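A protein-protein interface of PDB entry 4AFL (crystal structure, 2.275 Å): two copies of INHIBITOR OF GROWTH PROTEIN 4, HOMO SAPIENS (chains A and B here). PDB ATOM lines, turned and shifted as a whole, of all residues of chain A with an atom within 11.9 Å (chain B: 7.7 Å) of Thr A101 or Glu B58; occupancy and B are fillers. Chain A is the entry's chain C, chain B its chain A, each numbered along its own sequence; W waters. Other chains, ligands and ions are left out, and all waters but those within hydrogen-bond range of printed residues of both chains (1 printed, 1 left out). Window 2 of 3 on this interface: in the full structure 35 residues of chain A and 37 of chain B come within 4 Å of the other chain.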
ATOM      1  N   VAL A  92     -29.205 -14.124 -30.374  1.00  0.00           N
ATOM      2  CA  VAL A  92     -28.555 -13.354 -29.329  1.00  0.00           C
ATOM      3  C   VAL A  92     -27.927 -14.340 -28.331  1.00  0.00           C
ATOM      4  O   VAL A  92     -26.869 -14.086 -27.746  1.00  0.00           O
ATOM      5  CB  VAL A  92     -29.579 -12.467 -28.637  1.00  0.00           C
ATOM      6  CG1 VAL A  92     -28.982 -11.809 -27.412  1.00  0.00           C
ATOM      7  CG2 VAL A  92     -30.093 -11.426 -29.609  1.00  0.00           C
ATOM      8  N   ASP A  93     -28.560 -15.496 -28.176  1.00  0.00           N
ATOM      9  CA  ASP A  93     -28.077 -16.462 -27.209  1.00  0.00           C
ATOM     10  C   ASP A  93     -26.693 -16.982 -27.570  1.00  0.00           C
ATOM     11  O   ASP A  93     -25.867 -17.240 -26.692  1.00  0.00           O
ATOM     12  CB  ASP A  93     -29.052 -17.621 -27.066  1.00  0.00           C
ATOM     13  CG  ASP A  93     -28.795 -18.419 -25.806  1.00  0.00           C
ATOM     14  OD1 ASP A  93     -29.098 -17.909 -24.703  1.00  0.00           O
ATOM     15  OD2 ASP A  93     -28.260 -19.540 -25.915  1.00  0.00           O
ATOM     16  N   LYS A  94     -26.442 -17.146 -28.863  1.00  0.00           N
ATOM     17  CA  LYS A  94     -25.134 -17.591 -29.311  1.00  0.00           C
ATOM     18  C   LYS A  94     -24.065 -16.610 -28.848  1.00  0.00           C
ATOM     19  O   LYS A  94     -23.005 -17.015 -28.385  1.00  0.00           O
ATOM     20  CB  LYS A  94     -25.098 -17.740 -30.832  1.00  0.00           C
ATOM     21  CG  LYS A  94     -25.981 -18.853 -31.357  1.00  0.00           C
ATOM     22  CD  LYS A  94     -25.623 -19.204 -32.802  1.00  0.00           C
ATOM     23  CE  LYS A  94     -26.615 -20.194 -33.417  1.00  0.00           C
ATOM     24  NZ  LYS A  94     -27.969 -19.593 -33.617  1.00  0.00           N
ATOM     25  N   HIS A  95     -24.372 -15.319 -28.960  1.00  0.00           N
ATOM     26  CA  HIS A  95     -23.428 -14.261 -28.622  1.00  0.00           C
ATOM     27  C   HIS A  95     -23.238 -14.183 -27.128  1.00  0.00           C
ATOM     28  O   HIS A  95     -22.122 -14.016 -26.636  1.00  0.00           O
ATOM     29  CB  HIS A  95     -23.925 -12.913 -29.160  1.00  0.00           C
ATOM     30  CG  HIS A  95     -23.876 -12.816 -30.649  1.00  0.00           C
ATOM     31  ND1 HIS A  95     -22.690 -12.711 -31.339  1.00  0.00           N
ATOM     32  CD2 HIS A  95     -24.857 -12.851 -31.581  1.00  0.00           C
ATOM     33  CE1 HIS A  95     -22.944 -12.676 -32.637  1.00  0.00           C
ATOM     34  NE2 HIS A  95     -24.252 -12.753 -32.808  1.00  0.00           N
ATOM     35  N   ILE A  96     -24.338 -14.307 -26.403  1.00  0.00           N
ATOM     36  CA  ILE A  96     -24.272 -14.314 -24.949  1.00  0.00           C
ATOM     37  C   ILE A  96     -23.360 -15.434 -24.467  1.00  0.00           C
ATOM     38  O   ILE A  96     -22.526 -15.214 -23.606  1.00  0.00           O
ATOM     39  CB  ILE A  96     -25.670 -14.453 -24.324  1.00  0.00           C
ATOM     40  CG1 ILE A  96     -26.386 -13.105 -24.382  1.00  0.00           C
ATOM     41  CG2 ILE A  96     -25.586 -14.926 -22.876  1.00  0.00           C
ATOM     42  CD1 ILE A  96     -27.862 -13.220 -24.093  1.00  0.00           C
ATOM     43  N   ARG A  97     -23.517 -16.626 -25.030  1.00  0.00           N
ATOM     44  CA  ARG A  97     -22.678 -17.754 -24.635  1.00  0.00           C
ATOM     45  C   ARG A  97     -21.229 -17.460 -24.978  1.00  0.00           C
ATOM     46  O   ARG A  97     -20.335 -17.752 -24.186  1.00  0.00           O
ATOM     47  CB  ARG A  97     -23.142 -19.059 -25.291  1.00  0.00           C
ATOM     48  CG  ARG A  97     -24.222 -19.780 -24.490  1.00  0.00           C
ATOM     49  CD  ARG A  97     -25.242 -20.439 -25.395  1.00  0.00           C
ATOM     50  NE  ARG A  97     -25.366 -21.880 -25.169  1.00  0.00           N
ATOM     51  CZ  ARG A  97     -26.106 -22.438 -24.212  1.00  0.00           C
ATOM     52  NH1 ARG A  97     -26.785 -21.676 -23.361  1.00  0.00           N
ATOM     53  NH2 ARG A  97     -26.156 -23.763 -24.097  1.00  0.00           N
ATOM     54  N   ARG A  98     -21.014 -16.848 -26.143  1.00  0.00           N
ATOM     55  CA  ARG A  98     -19.668 -16.511 -26.598  1.00  0.00           C
ATOM     56  C   ARG A  98     -19.047 -15.476 -25.685  1.00  0.00           C
ATOM     57  O   ARG A  98     -17.877 -15.570 -25.313  1.00  0.00           O
ATOM     58  CB  ARG A  98     -19.671 -16.002 -28.051  1.00  0.00           C
ATOM     59  CG  ARG A  98     -18.312 -15.505 -28.542  1.00  0.00           C
ATOM     60  CD  ARG A  98     -18.366 -14.983 -29.994  1.00  0.00           C
ATOM     61  NE  ARG A  98     -19.336 -13.895 -30.129  1.00  0.00           N
ATOM     62  CZ  ARG A  98     -19.077 -12.610 -29.894  1.00  0.00           C
ATOM     63  NH1 ARG A  98     -17.860 -12.219 -29.516  1.00  0.00           N
ATOM     64  NH2 ARG A  98     -20.039 -11.710 -30.039  1.00  0.00           N
ATOM     65  N   LEU A  99     -19.835 -14.480 -25.317  1.00  0.00           N
ATOM     66  CA  LEU A  99     -19.302 -13.359 -24.556  1.00  0.00           C
ATOM     67  C   LEU A  99     -19.169 -13.661 -23.056  1.00  0.00           C
ATOM     68  O   LEU A  99     -18.335 -13.068 -22.371  1.00  0.00           O
ATOM     69  CB  LEU A  99     -20.175 -12.128 -24.751  1.00  0.00           C
ATOM     70  CG  LEU A  99     -20.245 -11.524 -26.153  1.00  0.00           C
ATOM     71  CD1 LEU A  99     -21.402 -10.514 -26.201  1.00  0.00           C
ATOM     72  CD2 LEU A  99     -18.913 -10.886 -26.582  1.00  0.00           C
ATOM     73  N   ASP A 100     -19.994 -14.559 -22.538  1.00  0.00           N
ATOM     74  CA  ASP A 100     -19.945 -14.840 -21.115  1.00  0.00           C
ATOM     75  C   ASP A 100     -18.706 -15.672 -20.799  1.00  0.00           C
ATOM     76  O   ASP A 100     -18.522 -16.762 -21.334  1.00  0.00           O
ATOM     77  CB  ASP A 100     -21.224 -15.532 -20.639  1.00  0.00           C
ATOM     78  CG  ASP A 100     -21.368 -15.514 -19.114  1.00  0.00           C
ATOM     79  OD1 ASP A 100     -20.458 -16.011 -18.416  1.00  0.00           O
ATOM     80  OD2 ASP A 100     -22.387 -14.990 -18.605  1.00  0.00           O
ATOM     81  N   THR A 101     -17.862 -15.135 -19.928  1.00  0.00           N
ATOM     82  CA  THR A 101     -16.649 -15.820 -19.466  1.00  0.00           C
ATOM     83  C   THR A 101     -16.908 -17.222 -18.917  1.00  0.00           C
ATOM     84  O   THR A 101     -16.013 -18.060 -18.936  1.00  0.00           O
ATOM     85  CB  THR A 101     -15.949 -15.019 -18.362  1.00  0.00           C
ATOM     86  OG1 THR A 101     -16.855 -14.839 -17.265  1.00  0.00           O
ATOM     87  CG2 THR A 101     -15.530 -13.654 -18.873  1.00  0.00           C
ATOM     88  N   ASP A 102     -18.119 -17.465 -18.414  1.00  0.00           N
ATOM     89  CA  ASP A 102     -18.496 -18.797 -17.949  1.00  0.00           C
ATOM     90  C   ASP A 102     -18.818 -19.708 -19.123  1.00  0.00           C
ATOM     91  O   ASP A 102     -18.319 -20.833 -19.197  1.00  0.00           O
ATOM     92  CB  ASP A 102     -19.680 -18.738 -16.987  1.00  0.00           C
ATOM     93  CG  ASP A 102     -19.429 -17.807 -15.814  1.00  0.00           C
ATOM     94  OD1 ASP A 102     -18.647 -18.183 -14.915  1.00  0.00           O
ATOM     95  OD2 ASP A 102     -20.012 -16.699 -15.793  1.00  0.00           O
ATOM     96  N   LEU A 103     -19.645 -19.213 -20.045  1.00  0.00           N
ATOM     97  CA  LEU A 103     -20.042 -19.986 -21.219  1.00  0.00           C
ATOM     98  C   LEU A 103     -18.994 -19.915 -22.337  1.00  0.00           C
ATOM     99  O   LEU A 103     -18.928 -20.811 -23.183  1.00  0.00           O
ATOM    100  CB  LEU A 103     -21.393 -19.532 -21.712  1.00  0.00           C
ATOM    101  N   ALA A 104     -18.199 -18.842 -22.342  1.00  0.00           N
ATOM    102  CA  ALA A 104     -17.003 -18.737 -23.190  1.00  0.00           C
ATOM    103  C   ALA A 104     -16.080 -17.605 -22.728  1.00  0.00           C
ATOM    104  O   ALA A 104     -15.346 -17.019 -23.525  1.00  0.00           O
ATOM    105  CB  ALA A 104     -17.369 -18.561 -24.661  1.00  0.00           C
ATOM    106  N   LEU B  55     -17.757  -1.572 -27.531  1.00  0.00           N
ATOM    107  CA  LEU B  55     -18.220  -1.973 -26.211  1.00  0.00           C
ATOM    108  C   LEU B  55     -17.381  -3.164 -25.796  1.00  0.00           C
ATOM    109  O   LEU B  55     -17.263  -4.119 -26.563  1.00  0.00           O
ATOM    110  CB  LEU B  55     -19.668  -2.465 -26.305  1.00  0.00           C
ATOM    111  CG  LEU B  55     -20.879  -1.543 -26.359  1.00  0.00           C
ATOM    112  CD1 LEU B  55     -22.108  -2.367 -26.743  1.00  0.00           C
ATOM    113  CD2 LEU B  55     -21.109  -0.825 -25.031  1.00  0.00           C
ATOM    114  N   SER B  56     -16.810  -3.144 -24.595  1.00  0.00           N
ATOM    115  CA  SER B  56     -16.063  -4.310 -24.144  1.00  0.00           C
ATOM    116  C   SER B  56     -17.058  -5.459 -23.977  1.00  0.00           C
ATOM    117  O   SER B  56     -18.270  -5.242 -23.933  1.00  0.00           O
ATOM    118  CB  SER B  56     -15.274  -4.039 -22.860  1.00  0.00           C
ATOM    119  OG  SER B  56     -16.074  -4.224 -21.709  1.00  0.00           O
ATOM    120  N   SER B  57     -16.552  -6.681 -23.924  1.00  0.00           N
ATOM    121  CA  SER B  57     -17.408  -7.857 -24.016  1.00  0.00           C
ATOM    122  C   SER B  57     -18.407  -7.919 -22.877  1.00  0.00           C
ATOM    123  O   SER B  57     -19.505  -8.422 -23.067  1.00  0.00           O
ATOM    124  CB  SER B  57     -16.580  -9.145 -24.083  1.00  0.00           C
ATOM    125  OG  SER B  57     -15.915  -9.363 -22.850  1.00  0.00           O
ATOM    126  N   GLU B  58     -18.047  -7.374 -21.713  1.00  0.00           N
ATOM    127  CA  GLU B  58     -18.954  -7.376 -20.569  1.00  0.00           C
ATOM    128  C   GLU B  58     -20.083  -6.378 -20.726  1.00  0.00           C
ATOM    129  O   GLU B  58     -21.195  -6.642 -20.284  1.00  0.00           O
ATOM    130  CB  GLU B  58     -18.216  -7.116 -19.245  1.00  0.00           C
ATOM    131  CG  GLU B  58     -17.401  -8.301 -18.748  1.00  0.00           C
ATOM    132  CD  GLU B  58     -18.260  -9.451 -18.242  1.00  0.00           C
ATOM    133  OE1 GLU B  58     -19.285  -9.177 -17.567  1.00  0.00           O
ATOM    134  OE2 GLU B  58     -17.903 -10.628 -18.511  1.00  0.00           O
ATOM    135  N   GLU B  59     -19.798  -5.231 -21.337  1.00  0.00           N
ATOM    136  CA  GLU B  59     -20.819  -4.202 -21.523  1.00  0.00           C
ATOM    137  C   GLU B  59     -21.802  -4.637 -22.613  1.00  0.00           C
ATOM    138  O   GLU B  59     -23.004  -4.430 -22.494  1.00  0.00           O
ATOM    139  CB  GLU B  59     -20.197  -2.844 -21.882  1.00  0.00           C
ATOM    140  CG  GLU B  59     -19.194  -2.294 -20.838  1.00  0.00           C
ATOM    141  CD  GLU B  59     -18.432  -1.040 -21.313  1.00  0.00           C
ATOM    142  OE1 GLU B  59     -17.627  -1.134 -22.276  1.00  0.00           O
ATOM    143  OE2 GLU B  59     -18.640   0.042 -20.716  1.00  0.00           O
ATOM    144  N   LYS B  60     -21.290  -5.247 -23.673  1.00  0.00           N
ATOM    145  CA  LYS B  60     -22.170  -5.780 -24.701  1.00  0.00           C
ATOM    146  C   LYS B  60     -23.003  -6.936 -24.132  1.00  0.00           C
ATOM    147  O   LYS B  60     -24.211  -7.024 -24.384  1.00  0.00           O
ATOM    148  CB  LYS B  60     -21.373  -6.259 -25.914  1.00  0.00           C
ATOM    149  CG  LYS B  60     -22.238  -6.752 -27.071  1.00  0.00           C
ATOM    150  CD  LYS B  60     -21.376  -7.020 -28.290  1.00  0.00           C
ATOM    151  CE  LYS B  60     -22.199  -7.391 -29.491  1.00  0.00           C
ATOM    152  NZ  LYS B  60     -21.311  -7.588 -30.670  1.00  0.00           N
ATOM    153  N   LEU B  61     -22.350  -7.820 -23.381  1.00  0.00           N
ATOM    154  CA  LEU B  61     -23.033  -8.953 -22.764  1.00  0.00           C
ATOM    155  C   LEU B  61     -24.234  -8.476 -21.959  1.00  0.00           C
ATOM    156  O   LEU B  61     -25.345  -8.972 -22.127  1.00  0.00           O
ATOM    157  CB  LEU B  61     -22.075  -9.784 -21.887  1.00  0.00           C
ATOM    158  CG  LEU B  61     -22.669 -10.885 -20.996  1.00  0.00           C
ATOM    159  CD1 LEU B  61     -23.422 -11.922 -21.809  1.00  0.00           C
ATOM    160  CD2 LEU B  61     -21.598 -11.581 -20.181  1.00  0.00           C
ATOM    161  N   ALA B  62     -24.022  -7.480 -21.114  1.00  0.00           N
ATOM    162  CA  ALA B  62     -25.098  -7.008 -20.249  1.00  0.00           C
ATOM    163  C   ALA B  62     -26.291  -6.483 -21.046  1.00  0.00           C
ATOM    164  O   ALA B  62     -27.421  -6.578 -20.600  1.00  0.00           O
ATOM    165  CB  ALA B  62     -24.592  -5.943 -19.318  1.00  0.00           C
ATOM    166  N   LEU B  63     -26.036  -5.923 -22.219  1.00  0.00           N
ATOM    167  CA  LEU B  63     -27.114  -5.393 -23.046  1.00  0.00           C
ATOM    168  C   LEU B  63     -27.885  -6.558 -23.664  1.00  0.00           C
ATOM    169  O   LEU B  63     -29.111  -6.628 -23.594  1.00  0.00           O
ATOM    170  CB  LEU B  63     -26.523  -4.531 -24.151  1.00  0.00           C
ATOM    171  CG  LEU B  63     -27.103  -3.145 -24.417  1.00  0.00           C
ATOM    172  CD1 LEU B  63     -27.773  -2.576 -23.176  1.00  0.00           C
ATOM    173  CD2 LEU B  63     -25.971  -2.232 -24.879  1.00  0.00           C
ATOM    174  N   LEU B  64     -27.138  -7.483 -24.250  1.00  0.00           N
ATOM    175  CA  LEU B  64     -27.708  -8.620 -24.932  1.00  0.00           C
ATOM    176  C   LEU B  64     -28.589  -9.456 -23.999  1.00  0.00           C
ATOM    177  O   LEU B  64     -29.658  -9.888 -24.410  1.00  0.00           O
ATOM    178  CB  LEU B  64     -26.594  -9.473 -25.542  1.00  0.00           C
ATOM    179  CG  LEU B  64     -25.813  -8.725 -26.620  1.00  0.00           C
ATOM    180  CD1 LEU B  64     -24.803  -9.635 -27.340  1.00  0.00           C
ATOM    181  CD2 LEU B  64     -26.780  -8.106 -27.623  1.00  0.00           C
HETATM  182  O   HOH W   1     -17.349 -10.935 -21.235  1.00  0.00           O
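The side-chain carboxylate of Asp A100 is in hydrogen-bond range of the backbone NH of Asp A102, 2.8 Å away. ND1 of His A95 is in hydrogen-bond range of NH2 of Arg A98 (3.1 Å).
Among the printed residues, pairs that only touch across the chains: Val A92 with Leu B64, Leu A99 with Leu B64, Asp A100 with Leu B61, Ile A96 with Leu B64, Leu A99 with Ser B57, His A95 with Leu B64, Ile A96 with Leu B61, Thr A101 with Glu B58 and Leu A99 with Lys B60.
Lys A94 touches none of the printed residues of chain B. Arg A97 touches none of the printed residues of chain B. Of the printed residues of chain B, Leu A99 touches Ser B57 (3.8 Å), Lys B60 (3.95 Å) and Leu B64 (3.7 Å). Of the printed residues of chain B, Asp A100 touches Leu B61 (3.8 Å). Of chain B, only Glu B58 (3.9 Å) comes within 4 Å of Thr A101. No residue of chain A comes within 4 Å of Ser B56. Glu B58 touches just one residue of chain A: Thr A101. No residue of chain A comes within 4 Å of Glu B59. Of the printed residues of chain A, Leu B61 touches Ile A96 (3.9 Å) and Asp A100 (3.8 Å). The nearest residue of chain B that does not touch Thr A101 is Leu B61 (5.2 Å). The nearest residue of chain A that does not touch Glu B58 is Leu A99 (4.6 Å).
Hydrophobic or aromatic side chains of chain B that line the printed part of chain A: Leu B61 and Leu B64. Printed residues of chain A that touch a printed residue of chain B: Val A92, His A95, Ile A96, Leu A99, Asp A100 and Thr A101. Hydrophobic or aromatic side chains of chain A that line the printed part of chain B: Val A92, His A95, Ile A96 and Leu A99.
No position is printed for both chains. Of the 9 pairs that touch across the chains among the printed residues, none has its exchanged pair printed and touching as well.
Water W1 lies within hydrogen-bond range of the backbone carbonyl oxygen (O) of Leu A99 (2.6 Å), the side-chain hydroxyl (OG) of Ser B57 (2.7 Å) and the side-chain carboxylate (OE2) of Glu B58 (2.8 Å).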
